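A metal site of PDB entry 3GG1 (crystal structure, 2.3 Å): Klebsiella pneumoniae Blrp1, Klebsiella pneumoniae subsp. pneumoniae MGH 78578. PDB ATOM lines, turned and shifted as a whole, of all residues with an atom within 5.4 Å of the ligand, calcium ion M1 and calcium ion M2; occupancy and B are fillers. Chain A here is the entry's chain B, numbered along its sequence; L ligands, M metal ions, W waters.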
ATOM      1  N   PHE A 179     -15.787 -17.030  -1.749  1.00  0.00           N
ATOM      2  CA  PHE A 179     -15.709 -15.818  -2.578  1.00  0.00           C
ATOM      3  C   PHE A 179     -16.280 -16.026  -3.980  1.00  0.00           C
ATOM      4  O   PHE A 179     -16.069 -17.065  -4.610  1.00  0.00           O
ATOM      5  CB  PHE A 179     -14.259 -15.328  -2.678  1.00  0.00           C
ATOM      6  CG  PHE A 179     -13.772 -14.663  -1.431  1.00  0.00           C
ATOM      7  CD1 PHE A 179     -13.189 -15.404  -0.416  1.00  0.00           C
ATOM      8  CD2 PHE A 179     -13.886 -13.288  -1.268  1.00  0.00           C
ATOM      9  CE1 PHE A 179     -12.736 -14.792   0.740  1.00  0.00           C
ATOM     10  CE2 PHE A 179     -13.436 -12.667  -0.114  1.00  0.00           C
ATOM     11  CZ  PHE A 179     -12.858 -13.421   0.898  1.00  0.00           C
ATOM     12  N   GLN A 182     -16.008 -11.592  -9.909  1.00  0.00           N
ATOM     13  CA  GLN A 182     -16.622 -10.845 -11.001  1.00  0.00           C
ATOM     14  C   GLN A 182     -15.538 -10.218 -11.856  1.00  0.00           C
ATOM     15  O   GLN A 182     -14.656  -9.516 -11.340  1.00  0.00           O
ATOM     16  CB  GLN A 182     -17.559  -9.755 -10.479  1.00  0.00           C
ATOM     17  CG  GLN A 182     -18.335  -9.046 -11.586  1.00  0.00           C
ATOM     18  CD  GLN A 182     -19.307  -8.002 -11.074  1.00  0.00           C
ATOM     19  OE1 GLN A 182     -19.089  -7.396 -10.024  1.00  0.00           O
ATOM     20  NE2 GLN A 182     -20.386  -7.785 -11.814  1.00  0.00           N
ATOM     21  N   GLU A 196     -12.537  -9.267  -9.407  1.00  0.00           N
ATOM     22  CA  GLU A 196     -12.756  -8.809  -8.035  1.00  0.00           C
ATOM     23  C   GLU A 196     -13.339  -9.937  -7.205  1.00  0.00           C
ATOM     24  O   GLU A 196     -14.346 -10.546  -7.586  1.00  0.00           O
ATOM     25  CB  GLU A 196     -13.690  -7.596  -8.014  1.00  0.00           C
ATOM     26  CG  GLU A 196     -13.948  -7.047  -6.607  1.00  0.00           C
ATOM     27  CD  GLU A 196     -14.891  -5.860  -6.591  1.00  0.00           C
ATOM     28  OE1 GLU A 196     -15.399  -5.471  -7.665  1.00  0.00           O
ATOM     29  OE2 GLU A 196     -15.122  -5.310  -5.483  1.00  0.00           O
ATOM     30  N   ALA A 197     -12.704 -10.225  -6.067  1.00  0.00           N
ATOM     31  CA  ALA A 197     -13.208 -11.202  -5.109  1.00  0.00           C
ATOM     32  C   ALA A 197     -14.215 -10.527  -4.186  1.00  0.00           C
ATOM     33  O   ALA A 197     -13.899  -9.530  -3.543  1.00  0.00           O
ATOM     34  CB  ALA A 197     -12.063 -11.804  -4.305  1.00  0.00           C
ATOM     35  N   LEU A 198     -15.422 -11.082  -4.127  1.00  0.00           N
ATOM     36  CA  LEU A 198     -16.492 -10.571  -3.265  1.00  0.00           C
ATOM     37  C   LEU A 198     -16.845 -11.672  -2.274  1.00  0.00           C
ATOM     38  O   LEU A 198     -17.151 -12.797  -2.665  1.00  0.00           O
ATOM     39  CB  LEU A 198     -17.728 -10.221  -4.099  1.00  0.00           C
ATOM     40  CG  LEU A 198     -17.540  -9.128  -5.165  1.00  0.00           C
ATOM     41  CD1 LEU A 198     -18.638  -9.219  -6.219  1.00  0.00           C
ATOM     42  CD2 LEU A 198     -17.503  -7.743  -4.528  1.00  0.00           C
ATOM     43  N   ILE A 199     -16.808 -11.336  -0.982  1.00  0.00           N
ATOM     44  CA  ILE A 199     -16.995 -12.335   0.073  1.00  0.00           C
ATOM     45  C   ILE A 199     -18.437 -12.855   0.120  1.00  0.00           C
ATOM     46  O   ILE A 199     -19.389 -12.110  -0.113  1.00  0.00           O
ATOM     47  CB  ILE A 199     -16.579 -11.783   1.464  1.00  0.00           C
ATOM     48  CG1 ILE A 199     -16.335 -12.930   2.440  1.00  0.00           C
ATOM     49  CG2 ILE A 199     -17.620 -10.790   2.005  1.00  0.00           C
ATOM     50  CD1 ILE A 199     -15.628 -12.516   3.725  1.00  0.00           C
ATOM     51  N   ARG A 200     -18.573 -14.145   0.413  1.00  0.00           N
ATOM     52  CA  ARG A 200     -19.875 -14.778   0.567  1.00  0.00           C
ATOM     53  C   ARG A 200     -19.891 -15.618   1.841  1.00  0.00           C
ATOM     54  O   ARG A 200     -18.859 -16.121   2.273  1.00  0.00           O
ATOM     55  CB  ARG A 200     -20.196 -15.648  -0.650  1.00  0.00           C
ATOM     56  CG  ARG A 200     -20.367 -14.879  -1.954  1.00  0.00           C
ATOM     57  CD  ARG A 200     -21.692 -14.133  -2.026  1.00  0.00           C
ATOM     58  NE  ARG A 200     -21.823 -13.391  -3.271  1.00  0.00           N
ATOM     59  CZ  ARG A 200     -21.383 -12.152  -3.487  1.00  0.00           C
ATOM     60  NH1 ARG A 200     -20.757 -11.468  -2.531  1.00  0.00           N
ATOM     61  NH2 ARG A 200     -21.554 -11.585  -4.675  1.00  0.00           N
ATOM     62  N   SER A 206     -24.782 -12.749   1.297  1.00  0.00           N
ATOM     63  CA  SER A 206     -24.072 -11.527   0.916  1.00  0.00           C
ATOM     64  C   SER A 206     -23.016 -11.141   1.956  1.00  0.00           C
ATOM     65  O   SER A 206     -22.998 -11.694   3.052  1.00  0.00           O
ATOM     66  CB  SER A 206     -25.085 -10.385   0.727  1.00  0.00           C
ATOM     67  OG  SER A 206     -25.609  -9.950   1.974  1.00  0.00           O
ATOM     68  N   PRO A 207     -22.123 -10.184   1.603  1.00  0.00           N
ATOM     69  CA  PRO A 207     -21.145  -9.677   2.573  1.00  0.00           C
ATOM     70  C   PRO A 207     -21.763  -9.144   3.880  1.00  0.00           C
ATOM     71  O   PRO A 207     -21.155  -9.265   4.933  1.00  0.00           O
ATOM     72  CB  PRO A 207     -20.454  -8.542   1.808  1.00  0.00           C
ATOM     73  CG  PRO A 207     -20.602  -8.909   0.391  1.00  0.00           C
ATOM     74  CD  PRO A 207     -21.945  -9.556   0.287  1.00  0.00           C
ATOM     75  N   PHE A 211     -20.651 -10.828   7.521  1.00  0.00           N
ATOM     76  CA  PHE A 211     -20.094 -10.031   8.611  1.00  0.00           C
ATOM     77  C   PHE A 211     -21.039  -9.915   9.805  1.00  0.00           C
ATOM     78  O   PHE A 211     -20.578  -9.778  10.944  1.00  0.00           O
ATOM     79  CB  PHE A 211     -19.672  -8.641   8.116  1.00  0.00           C
ATOM     80  CG  PHE A 211     -18.324  -8.624   7.467  1.00  0.00           C
ATOM     81  CD1 PHE A 211     -17.174  -8.628   8.237  1.00  0.00           C
ATOM     82  CD2 PHE A 211     -18.204  -8.612   6.081  1.00  0.00           C
ATOM     83  CE1 PHE A 211     -15.924  -8.611   7.645  1.00  0.00           C
ATOM     84  CE2 PHE A 211     -16.957  -8.586   5.488  1.00  0.00           C
ATOM     85  CZ  PHE A 211     -15.820  -8.594   6.262  1.00  0.00           C
ATOM     86  N   ASP A 223     -12.059  -9.975   8.260  1.00  0.00           N
ATOM     87  CA  ASP A 223     -11.989  -9.387   6.926  1.00  0.00           C
ATOM     88  C   ASP A 223     -10.611  -9.621   6.318  1.00  0.00           C
ATOM     89  O   ASP A 223     -10.499 -10.117   5.197  1.00  0.00           O
ATOM     90  CB  ASP A 223     -12.302  -7.884   7.004  1.00  0.00           C
ATOM     91  CG  ASP A 223     -12.409  -7.233   5.645  1.00  0.00           C
ATOM     92  OD1 ASP A 223     -12.669  -7.942   4.640  1.00  0.00           O
ATOM     93  OD2 ASP A 223     -12.255  -5.998   5.573  1.00  0.00           O
ATOM     94  N   SER A 226      -9.953 -13.532   6.019  1.00  0.00           N
ATOM     95  CA  SER A 226     -10.795 -14.163   5.002  1.00  0.00           C
ATOM     96  C   SER A 226     -10.090 -14.224   3.641  1.00  0.00           C
ATOM     97  O   SER A 226     -10.379 -15.105   2.840  1.00  0.00           O
ATOM     98  CB  SER A 226     -12.127 -13.413   4.856  1.00  0.00           C
ATOM     99  OG  SER A 226     -11.925 -12.062   4.486  1.00  0.00           O
ATOM    100  N   LYS A 227      -9.158 -13.303   3.417  1.00  0.00           N
ATOM    101  CA  LYS A 227      -8.475 -13.164   2.124  1.00  0.00           C
ATOM    102  C   LYS A 227      -7.591 -14.350   1.746  1.00  0.00           C
ATOM    103  O   LYS A 227      -7.280 -14.518   0.581  1.00  0.00           O
ATOM    104  CB  LYS A 227      -7.652 -11.874   2.090  1.00  0.00           C
ATOM    105  CG  LYS A 227      -8.472 -10.597   2.332  1.00  0.00           C
ATOM    106  CD  LYS A 227      -9.582 -10.428   1.305  1.00  0.00           C
ATOM    107  CE  LYS A 227     -10.597  -9.414   1.745  1.00  0.00           C
ATOM    108  NZ  LYS A 227     -11.636  -9.975   2.639  1.00  0.00           N
ATOM    109  N   ASN A 247     -11.363  -6.695  -1.376  1.00  0.00           N
ATOM    110  CA  ASN A 247     -11.962  -5.598  -0.606  1.00  0.00           C
ATOM    111  C   ASN A 247     -11.555  -5.659   0.862  1.00  0.00           C
ATOM    112  O   ASN A 247     -11.678  -6.709   1.513  1.00  0.00           O
ATOM    113  CB  ASN A 247     -13.479  -5.658  -0.710  1.00  0.00           C
ATOM    114  CG  ASN A 247     -13.973  -5.387  -2.114  1.00  0.00           C
ATOM    115  OD1 ASN A 247     -14.103  -4.232  -2.508  1.00  0.00           O
ATOM    116  ND2 ASN A 247     -14.238  -6.446  -2.877  1.00  0.00           N
ATOM    117  N   LEU A 248     -11.077  -4.543   1.392  1.00  0.00           N
ATOM    118  CA  LEU A 248     -10.734  -4.432   2.809  1.00  0.00           C
ATOM    119  C   LEU A 248     -11.174  -3.081   3.348  1.00  0.00           C
ATOM    120  O   LEU A 248     -11.035  -2.063   2.672  1.00  0.00           O
ATOM    121  CB  LEU A 248      -9.224  -4.591   3.015  1.00  0.00           C
ATOM    122  CG  LEU A 248      -8.640  -6.002   2.935  1.00  0.00           C
ATOM    123  CD1 LEU A 248      -7.119  -5.964   2.925  1.00  0.00           C
ATOM    124  CD2 LEU A 248      -9.135  -6.857   4.097  1.00  0.00           C
ATOM    125  N   LEU A 249     -11.714  -3.079   4.563  1.00  0.00           N
ATOM    126  CA  LEU A 249     -11.953  -1.854   5.304  1.00  0.00           C
ATOM    127  C   LEU A 249     -10.613  -1.331   5.803  1.00  0.00           C
ATOM    128  O   LEU A 249      -9.704  -2.124   6.081  1.00  0.00           O
ATOM    129  CB  LEU A 249     -12.894  -2.096   6.478  1.00  0.00           C
ATOM    130  CG  LEU A 249     -14.335  -2.460   6.128  1.00  0.00           C
ATOM    131  CD1 LEU A 249     -15.036  -3.149   7.294  1.00  0.00           C
ATOM    132  CD2 LEU A 249     -15.105  -1.222   5.688  1.00  0.00           C
ATOM    133  N   GLU A 280      -8.883  -2.858  -2.694  1.00  0.00           N
ATOM    134  CA  GLU A 280      -9.950  -1.874  -2.880  1.00  0.00           C
ATOM    135  C   GLU A 280     -10.454  -1.387  -1.516  1.00  0.00           C
ATOM    136  O   GLU A 280     -10.943  -2.175  -0.711  1.00  0.00           O
ATOM    137  CB  GLU A 280     -11.099  -2.470  -3.684  1.00  0.00           C
ATOM    138  CG  GLU A 280     -10.658  -3.061  -5.027  1.00  0.00           C
ATOM    139  CD  GLU A 280     -11.792  -3.260  -6.021  1.00  0.00           C
ATOM    140  OE1 GLU A 280     -11.490  -3.520  -7.204  1.00  0.00           O
ATOM    141  OE2 GLU A 280     -12.971  -3.157  -5.643  1.00  0.00           O
ATOM    142  N   THR A 282     -12.929   1.609   0.354  1.00  0.00           N
ATOM    143  CA  THR A 282     -14.033   2.545   0.100  1.00  0.00           C
ATOM    144  C   THR A 282     -13.616   3.991   0.347  1.00  0.00           C
ATOM    145  O   THR A 282     -12.989   4.291   1.375  1.00  0.00           O
ATOM    146  CB  THR A 282     -15.249   2.209   0.969  1.00  0.00           C
ATOM    147  OG1 THR A 282     -14.819   1.936   2.311  1.00  0.00           O
ATOM    148  CG2 THR A 282     -15.963   0.980   0.438  1.00  0.00           C
ATOM    149  N   ASP A 310     -12.353   2.664  -3.872  1.00  0.00           N
ATOM    150  CA  ASP A 310     -13.617   2.027  -4.220  1.00  0.00           C
ATOM    151  C   ASP A 310     -14.765   3.014  -4.000  1.00  0.00           C
ATOM    152  O   ASP A 310     -14.586   4.033  -3.334  1.00  0.00           O
ATOM    153  CB  ASP A 310     -13.810   0.797  -3.331  1.00  0.00           C
ATOM    154  CG  ASP A 310     -14.672  -0.269  -3.974  1.00  0.00           C
ATOM    155  OD1 ASP A 310     -14.700  -1.397  -3.441  1.00  0.00           O
ATOM    156  OD2 ASP A 310     -15.308  -0.003  -5.008  1.00  0.00           O
ATOM    157  N   ASP A 311     -15.925   2.701  -4.566  1.00  0.00           N
ATOM    158  CA  ASP A 311     -17.145   3.491  -4.342  1.00  0.00           C
ATOM    159  C   ASP A 311     -16.914   4.987  -4.579  1.00  0.00           C
ATOM    160  O   ASP A 311     -17.391   5.833  -3.817  1.00  0.00           O
ATOM    161  CB  ASP A 311     -17.682   3.268  -2.915  1.00  0.00           C
ATOM    162  CG  ASP A 311     -18.124   1.831  -2.664  1.00  0.00           C
ATOM    163  OD1 ASP A 311     -18.318   1.067  -3.631  1.00  0.00           O
ATOM    164  OD2 ASP A 311     -18.292   1.459  -1.482  1.00  0.00           O
ATOM    165  N   LYS A 331     -12.512   3.432  -8.829  1.00  0.00           N
ATOM    166  CA  LYS A 331     -13.695   2.731  -9.304  1.00  0.00           C
ATOM    167  C   LYS A 331     -14.917   3.627  -9.139  1.00  0.00           C
ATOM    168  O   LYS A 331     -15.372   3.856  -8.013  1.00  0.00           O
ATOM    169  CB  LYS A 331     -13.883   1.422  -8.551  1.00  0.00           C
ATOM    170  CG  LYS A 331     -12.667   0.525  -8.661  1.00  0.00           C
ATOM    171  CD  LYS A 331     -12.915  -0.845  -8.096  1.00  0.00           C
ATOM    172  CE  LYS A 331     -13.649  -1.745  -9.082  1.00  0.00           C
ATOM    173  NZ  LYS A 331     -13.981  -3.057  -8.463  1.00  0.00           N
ATOM    174  N   ASP A 333     -18.473   4.713  -8.753  1.00  0.00           N
ATOM    175  CA  ASP A 333     -19.576   3.985  -8.142  1.00  0.00           C
ATOM    176  C   ASP A 333     -20.769   3.864  -9.078  1.00  0.00           C
ATOM    177  O   ASP A 333     -20.990   4.718  -9.946  1.00  0.00           O
ATOM    178  CB  ASP A 333     -20.016   4.645  -6.833  1.00  0.00           C
ATOM    179  CG  ASP A 333     -20.897   3.740  -5.995  1.00  0.00           C
ATOM    180  OD1 ASP A 333     -20.395   2.694  -5.530  1.00  0.00           O
ATOM    181  OD2 ASP A 333     -22.092   4.050  -5.837  1.00  0.00           O
ATOM    182  N   ALA A 334     -21.540   2.798  -8.885  1.00  0.00           N
ATOM    183  CA  ALA A 334     -22.753   2.542  -9.658  1.00  0.00           C
ATOM    184  C   ALA A 334     -23.743   3.709  -9.612  1.00  0.00           C
ATOM    185  O   ALA A 334     -24.467   3.928 -10.570  1.00  0.00           O
ATOM    186  CB  ALA A 334     -23.423   1.259  -9.171  1.00  0.00           C
ATOM    187  N   ARG A 338     -25.682   4.934 -12.792  1.00  0.00           N
ATOM    188  CA  ARG A 338     -27.130   4.857 -12.936  1.00  0.00           C
ATOM    189  C   ARG A 338     -27.684   6.049 -13.701  1.00  0.00           C
ATOM    190  O   ARG A 338     -27.457   7.197 -13.322  1.00  0.00           O
ATOM    191  CB  ARG A 338     -27.835   4.811 -11.575  1.00  0.00           C
ATOM    192  CG  ARG A 338     -27.654   3.521 -10.823  1.00  0.00           C
ATOM    193  CD  ARG A 338     -28.513   2.397 -11.382  1.00  0.00           C
ATOM    194  NE  ARG A 338     -27.893   1.115 -11.056  1.00  0.00           N
ATOM    195  CZ  ARG A 338     -27.014   0.461 -11.823  1.00  0.00           C
ATOM    196  NH1 ARG A 338     -26.640   0.949 -12.998  1.00  0.00           N
ATOM    197  NH2 ARG A 338     -26.516  -0.691 -11.394  1.00  0.00           N
ATOM    198  N   GLU A 367     -18.286   0.746 -12.482  1.00  0.00           N
ATOM    199  CA  GLU A 367     -18.910  -0.470 -11.956  1.00  0.00           C
ATOM    200  C   GLU A 367     -20.427  -0.361 -11.920  1.00  0.00           C
ATOM    201  O   GLU A 367     -20.996   0.732 -11.995  1.00  0.00           O
ATOM    202  CB  GLU A 367     -18.349  -0.808 -10.570  1.00  0.00           C
ATOM    203  CG  GLU A 367     -18.974  -0.061  -9.419  1.00  0.00           C
ATOM    204  CD  GLU A 367     -18.101  -0.096  -8.184  1.00  0.00           C
ATOM    205  OE1 GLU A 367     -18.043   0.925  -7.464  1.00  0.00           O
ATOM    206  OE2 GLU A 367     -17.463  -1.138  -7.929  1.00  0.00           O
ATOM    207  N   GLY A 368     -21.086  -1.516 -11.824  1.00  0.00           N
ATOM    208  CA  GLY A 368     -22.538  -1.585 -11.819  1.00  0.00           C
ATOM    209  C   GLY A 368     -23.160  -1.294 -13.171  1.00  0.00           C
ATOM    210  O   GLY A 368     -24.285  -0.778 -13.228  1.00  0.00           O
ATOM    211  N   VAL A 369     -22.462  -1.613 -14.256  1.00  0.00           N
ATOM    212  CA  VAL A 369     -22.990  -1.374 -15.599  1.00  0.00           C
ATOM    213  C   VAL A 369     -23.987  -2.464 -15.973  1.00  0.00           C
ATOM    214  O   VAL A 369     -23.611  -3.628 -16.130  1.00  0.00           O
ATOM    215  CB  VAL A 369     -21.858  -1.312 -16.658  1.00  0.00           C
ATOM    216  CG1 VAL A 369     -22.439  -1.102 -18.055  1.00  0.00           C
ATOM    217  CG2 VAL A 369     -20.875  -0.201 -16.316  1.00  0.00           C
ATOM    218  N   GLU A 370     -25.261  -2.082 -16.119  1.00  0.00           N
ATOM    219  CA  GLU A 370     -26.354  -3.027 -16.364  1.00  0.00           C
ATOM    220  C   GLU A 370     -26.919  -2.992 -17.798  1.00  0.00           C
ATOM    221  O   GLU A 370     -27.488  -3.984 -18.254  1.00  0.00           O
ATOM    222  CB  GLU A 370     -27.495  -2.772 -15.370  1.00  0.00           C
ATOM    223  CG  GLU A 370     -27.168  -3.193 -13.949  1.00  0.00           C
ATOM    224  CD  GLU A 370     -28.213  -2.730 -12.944  1.00  0.00           C
ATOM    225  OE1 GLU A 370     -28.107  -3.126 -11.760  1.00  0.00           O
ATOM    226  OE2 GLU A 370     -29.123  -1.965 -13.303  1.00  0.00           O
ATOM    227  N   GLN A 387     -17.280  -2.977 -15.254  1.00  0.00           N
ATOM    228  CA  GLN A 387     -17.693  -4.056 -14.369  1.00  0.00           C
ATOM    229  C   GLN A 387     -19.201  -3.982 -14.153  1.00  0.00           C
ATOM    230  O   GLN A 387     -19.720  -2.943 -13.743  1.00  0.00           O
ATOM    231  CB  GLN A 387     -16.964  -3.924 -13.023  1.00  0.00           C
ATOM    232  CG  GLN A 387     -17.176  -5.083 -12.076  1.00  0.00           C
ATOM    233  CD  GLN A 387     -16.374  -4.949 -10.791  1.00  0.00           C
ATOM    234  OE1 GLN A 387     -15.662  -3.957 -10.576  1.00  0.00           O
ATOM    235  NE2 GLN A 387     -16.461  -5.964  -9.933  1.00  0.00           N
ATOM    236  N   GLY A 388     -19.914  -5.055 -14.450  1.00  0.00           N
ATOM    237  CA  GLY A 388     -21.374  -5.058 -14.275  1.00  0.00           C
ATOM    238  C   GLY A 388     -22.094  -6.269 -14.810  1.00  0.00           C
ATOM    239  O   GLY A 388     -21.535  -7.054 -15.569  1.00  0.00           O
ATOM    240  N   PHE A 389     -23.365  -6.402 -14.429  1.00  0.00           N
ATOM    241  CA  PHE A 389     -24.198  -7.539 -14.832  1.00  0.00           C
ATOM    242  C   PHE A 389     -24.394  -7.639 -16.337  1.00  0.00           C
ATOM    243  O   PHE A 389     -24.714  -8.708 -16.853  1.00  0.00           O
ATOM    244  CB  PHE A 389     -25.576  -7.474 -14.154  1.00  0.00           C
ATOM    245  CG  PHE A 389     -25.549  -7.636 -12.646  1.00  0.00           C
ATOM    246  CD1 PHE A 389     -24.407  -8.061 -11.973  1.00  0.00           C
ATOM    247  CD2 PHE A 389     -26.697  -7.383 -11.912  1.00  0.00           C
ATOM    248  CE1 PHE A 389     -24.413  -8.207 -10.589  1.00  0.00           C
ATOM    249  CE2 PHE A 389     -26.719  -7.536 -10.537  1.00  0.00           C
ATOM    250  CZ  PHE A 389     -25.570  -7.939  -9.872  1.00  0.00           C
ATOM    251  N   LEU A 390     -24.217  -6.519 -17.049  1.00  0.00           N
ATOM    252  CA  LEU A 390     -24.270  -6.519 -18.514  1.00  0.00           C
ATOM    253  C   LEU A 390     -23.248  -7.490 -19.125  1.00  0.00           C
ATOM    254  O   LEU A 390     -23.524  -8.139 -20.128  1.00  0.00           O
ATOM    255  CB  LEU A 390     -24.002  -5.116 -19.055  1.00  0.00           C
ATOM    256  CG  LEU A 390     -24.125  -4.924 -20.575  1.00  0.00           C
ATOM    257  CD1 LEU A 390     -25.554  -5.160 -21.046  1.00  0.00           C
ATOM    258  CD2 LEU A 390     -23.644  -3.525 -20.965  1.00  0.00           C
ATOM    259  N   PRO A 394     -21.148 -11.839 -10.761  1.00  0.00           N
ATOM    260  CA  PRO A 394     -20.278 -12.539  -9.819  1.00  0.00           C
ATOM    261  C   PRO A 394     -20.462 -14.062  -9.892  1.00  0.00           C
ATOM    262  O   PRO A 394     -21.600 -14.541  -9.944  1.00  0.00           O
ATOM    263  CB  PRO A 394     -20.730 -12.024  -8.459  1.00  0.00           C
ATOM    264  CG  PRO A 394     -21.397 -10.737  -8.732  1.00  0.00           C
ATOM    265  CD  PRO A 394     -21.984 -10.824 -10.097  1.00  0.00           C
HETATM  266  P1  LIG L   1     -18.533  -3.175  -4.079  1.00  0.00           P
HETATM  267  O1  LIG L   1     -17.068  -3.238  -3.750  1.00  0.00           O
HETATM  268  O2  LIG L   1     -19.105  -1.967  -4.785  1.00  0.00           O
HETATM  269  O3  LIG L   1     -18.906  -4.511  -4.907  1.00  0.00           O
HETATM  270  C1  LIG L   1     -19.788  -4.520  -6.029  1.00  0.00           C
HETATM  271  C2  LIG L   1     -21.172  -4.997  -5.610  1.00  0.00           C
HETATM  272  O4  LIG L   1     -22.100  -4.635  -6.633  1.00  0.00           O
HETATM  273  C3  LIG L   1     -21.272  -6.510  -5.516  1.00  0.00           C
HETATM  274  O5  LIG L   1     -22.278  -6.899  -4.580  1.00  0.00           O
HETATM  275  C4  LIG L   1     -21.724  -6.885  -6.882  1.00  0.00           C
HETATM  276  O6  LIG L   1     -22.091  -8.138  -7.112  1.00  0.00           O
HETATM  277  C5  LIG L   1     -22.384  -5.840  -7.396  1.00  0.00           C
HETATM  278  N1  LIG L   1     -22.582  -5.660  -8.739  1.00  0.00           N
HETATM  279  C6  LIG L   1     -21.729  -5.943  -9.649  1.00  0.00           C
HETATM  280  N2  LIG L   1     -22.232  -5.610 -10.791  1.00  0.00           N
HETATM  281  C7  LIG L   1     -23.463  -5.064 -10.631  1.00  0.00           C
HETATM  282  C8  LIG L   1     -24.442  -4.553 -11.475  1.00  0.00           C
HETATM  283  O7  LIG L   1     -24.284  -4.496 -12.709  1.00  0.00           O
HETATM  284  N3  LIG L   1     -25.585  -4.077 -10.924  1.00  0.00           N
HETATM  285  C9  LIG L   1     -25.793  -4.117  -9.580  1.00  0.00           C
HETATM  286  N4  LIG L   1     -26.953  -3.639  -9.087  1.00  0.00           N
HETATM  287  N5  LIG L   1     -24.854  -4.621  -8.737  1.00  0.00           N
HETATM  288  C10 LIG L   1     -23.684  -5.100  -9.248  1.00  0.00           C
HETATM  289  P2  LIG L   1     -21.916  -7.450  -3.114  1.00  0.00           P
HETATM  290  O8  LIG L   1     -23.226  -8.194  -2.546  1.00  0.00           O
HETATM  291  O9  LIG L   1     -20.828  -8.584  -3.371  1.00  0.00           O
HETATM  292  O10 LIG L   1     -21.106  -6.470  -2.130  1.00  0.00           O
HETATM  293  C11 LIG L   1     -21.658  -5.313  -1.506  1.00  0.00           C
HETATM  294  C12 LIG L   1     -20.370  -4.730  -0.945  1.00  0.00           C
HETATM  295  O11 LIG L   1     -19.786  -5.544   0.082  1.00  0.00           O
HETATM  296  C13 LIG L   1     -19.246  -4.544  -1.963  1.00  0.00           C
HETATM  297  O12 LIG L   1     -19.355  -3.335  -2.706  1.00  0.00           O
HETATM  298  C14 LIG L   1     -18.019  -4.601  -1.111  1.00  0.00           C
HETATM  299  O13 LIG L   1     -17.904  -3.443  -0.449  1.00  0.00           O
HETATM  300  C15 LIG L   1     -18.383  -5.569  -0.290  1.00  0.00           C
HETATM  301  N6  LIG L   1     -17.510  -6.572   0.024  1.00  0.00           N
HETATM  302  C16 LIG L   1     -17.462  -7.671  -0.726  1.00  0.00           C
HETATM  303  N7  LIG L   1     -16.492  -8.430  -0.179  1.00  0.00           N
HETATM  304  C17 LIG L   1     -15.956  -7.756   0.875  1.00  0.00           C
HETATM  305  C18 LIG L   1     -14.943  -8.061   1.774  1.00  0.00           C
HETATM  306  O14 LIG L   1     -14.331  -9.150   1.688  1.00  0.00           O
HETATM  307  N8  LIG L   1     -14.638  -7.171   2.748  1.00  0.00           N
HETATM  308  C19 LIG L   1     -15.298  -5.988   2.841  1.00  0.00           C
HETATM  309  N9  LIG L   1     -14.962  -5.118   3.822  1.00  0.00           N
HETATM  310  N10 LIG L   1     -16.289  -5.669   1.978  1.00  0.00           N
HETATM  311  C20 LIG L   1     -16.625  -6.539   0.997  1.00  0.00           C
HETATM  312 CA    CA M   1     -19.594   0.261  -5.338  1.00  0.00          CA
HETATM  313 CA    CA M   2     -14.957  -3.283  -4.513  1.00  0.00          CA
HETATM  314  O   HOH W   1     -25.988  -6.125  -6.314  1.00  0.00           O
HETATM  315  O   HOH W   2     -16.185  -2.786  -6.462  1.00  0.00           O
HETATM  316  O   HOH W   3     -12.918  -9.203  -1.009  1.00  0.00           O
HETATM  317  O   HOH W   4     -16.790  -1.240  -1.604  1.00  0.00           O
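OD1 of Asp 311 binds calcium ion M1 (2.3 Å).
Calcium ion M1 is bound by O2 of the ligand (2.3 Å).
Calcium ion M1 is bound by OD1 of Asp 333, 2.6 Å away.
Calcium ion M1 is bound by OE1 of Glu 367 (2.7 Å).
Of the 33 residues printed, 3 come within 4 Å of calcium ion M1.
The nearest printed residue that does not touch calcium ion M1 is Asp 310 (4.3 Å).
Water W4 bridges O13 of the ligand (2.7 Å) and OD2 of Asp 311 (3.1 Å).
Water W3 lies within hydrogen-bond range of the backbone carbonyl oxygen of Ala 197, the backbone NH of Asn 247 and an oxygen (O14) of the ligand.
OE1 of Glu 370 is in salt-bridge range of NH2 of Arg 338, at 2.9 Å.
N of Leu 390 is in hydrogen-bond range of O of Val 369 (3.1 Å).
The backbone carbonyl oxygen of Gln 182 lies within hydrogen-bond range of the backbone NH of Glu 196 (2.9 Å).
NZ of Lys 227 sits close to O of Asn 247, at 3.5 Å.
The side-chain carboxylate of Asp 223 lies within salt-bridge range of the side-chain amino group of Lys 227 (3.0 Å).
The side-chain carboxylate of Glu 196 is in hydrogen-bond range of the side-chain amide nitrogen of Gln 387.
The backbone carbonyl oxygen (O) of Val 369 lies within hydrogen-bond range of the backbone NH (N) of Phe 389 (3.3 Å).
The backbone carbonyl oxygen (O) of Glu 280 is in hydrogen-bond range of the backbone NH (N) of Leu 248.
Calcium ion M2 is bound by OD1 of Asp 310 (2.2 Å), O1 of the ligand (2.2 Å), OE2 of Glu 196 (2.3 Å), OE2 of Glu 280 (2.3 Å), water W2 (2.4 Å) and OD1 of Asn 247 (2.4 Å).
Within 4 Å of calcium ion M2: Glu 196, Asn 247, Glu 280 and Asp 310.
A nitrogen (N8) of the ligand sits at hydrogen-bond distance from the backbone carbonyl oxygen of Asn 247 (3.2 Å).
OD1 of Asp 223 is in hydrogen-bond range of N8 of the ligand, 2.8 Å away.
The backbone NH (N) of Phe 389 is in hydrogen-bond range of an oxygen (O7) of the ligand.
OE1 of Glu 370 sits at hydrogen-bond distance from N3 of the ligand (2.8 Å).
NE2 of Gln 182 lies within hydrogen-bond range of N2 of the ligand (3.0 Å).
The guanidinium group (NH1) of Arg 200 is in salt-bridge range of an oxygen (O9) of the ligand (3.0 Å).
A nitrogen (N7) of the ligand lies within hydrogen-bond range of the backbone NH (N) of Ile 199 (3.0 Å).
An oxygen (O14) of the ligand is in hydrogen-bond range of the side-chain amino group (NZ) of Lys 227, at 3.0 Å.
Merely in contact with the ligand: Pro 394 (3.1 Å), Gly 388 (3.4 Å), Pro 207 (3.4 Å), Gly 368 (3.4 Å), Arg 338 (3.5 Å), Leu 198 (3.5 Å), Leu 249 (3.6 Å), Val 369 (3.6 Å) and Phe 211 (3.9 Å).
Hydrophobic or aromatic side chains within 4 Å of the ligand: Leu 198, Ile 199, Pro 207, Phe 211, Leu 249, Phe 389 and Pro 394.
21 residues have an atom within 4 Å of the ligand: Gln 182, Glu 196, Leu 198, Ile 199, Arg 200, Pro 207, Phe 211, Asp 223, Lys 227, Asn 247, Leu 249, Asp 310, Asp 311, Arg 338, Glu 367, Gly 368, Val 369, Glu 370, Gly 388, Phe 389 and Pro 394.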
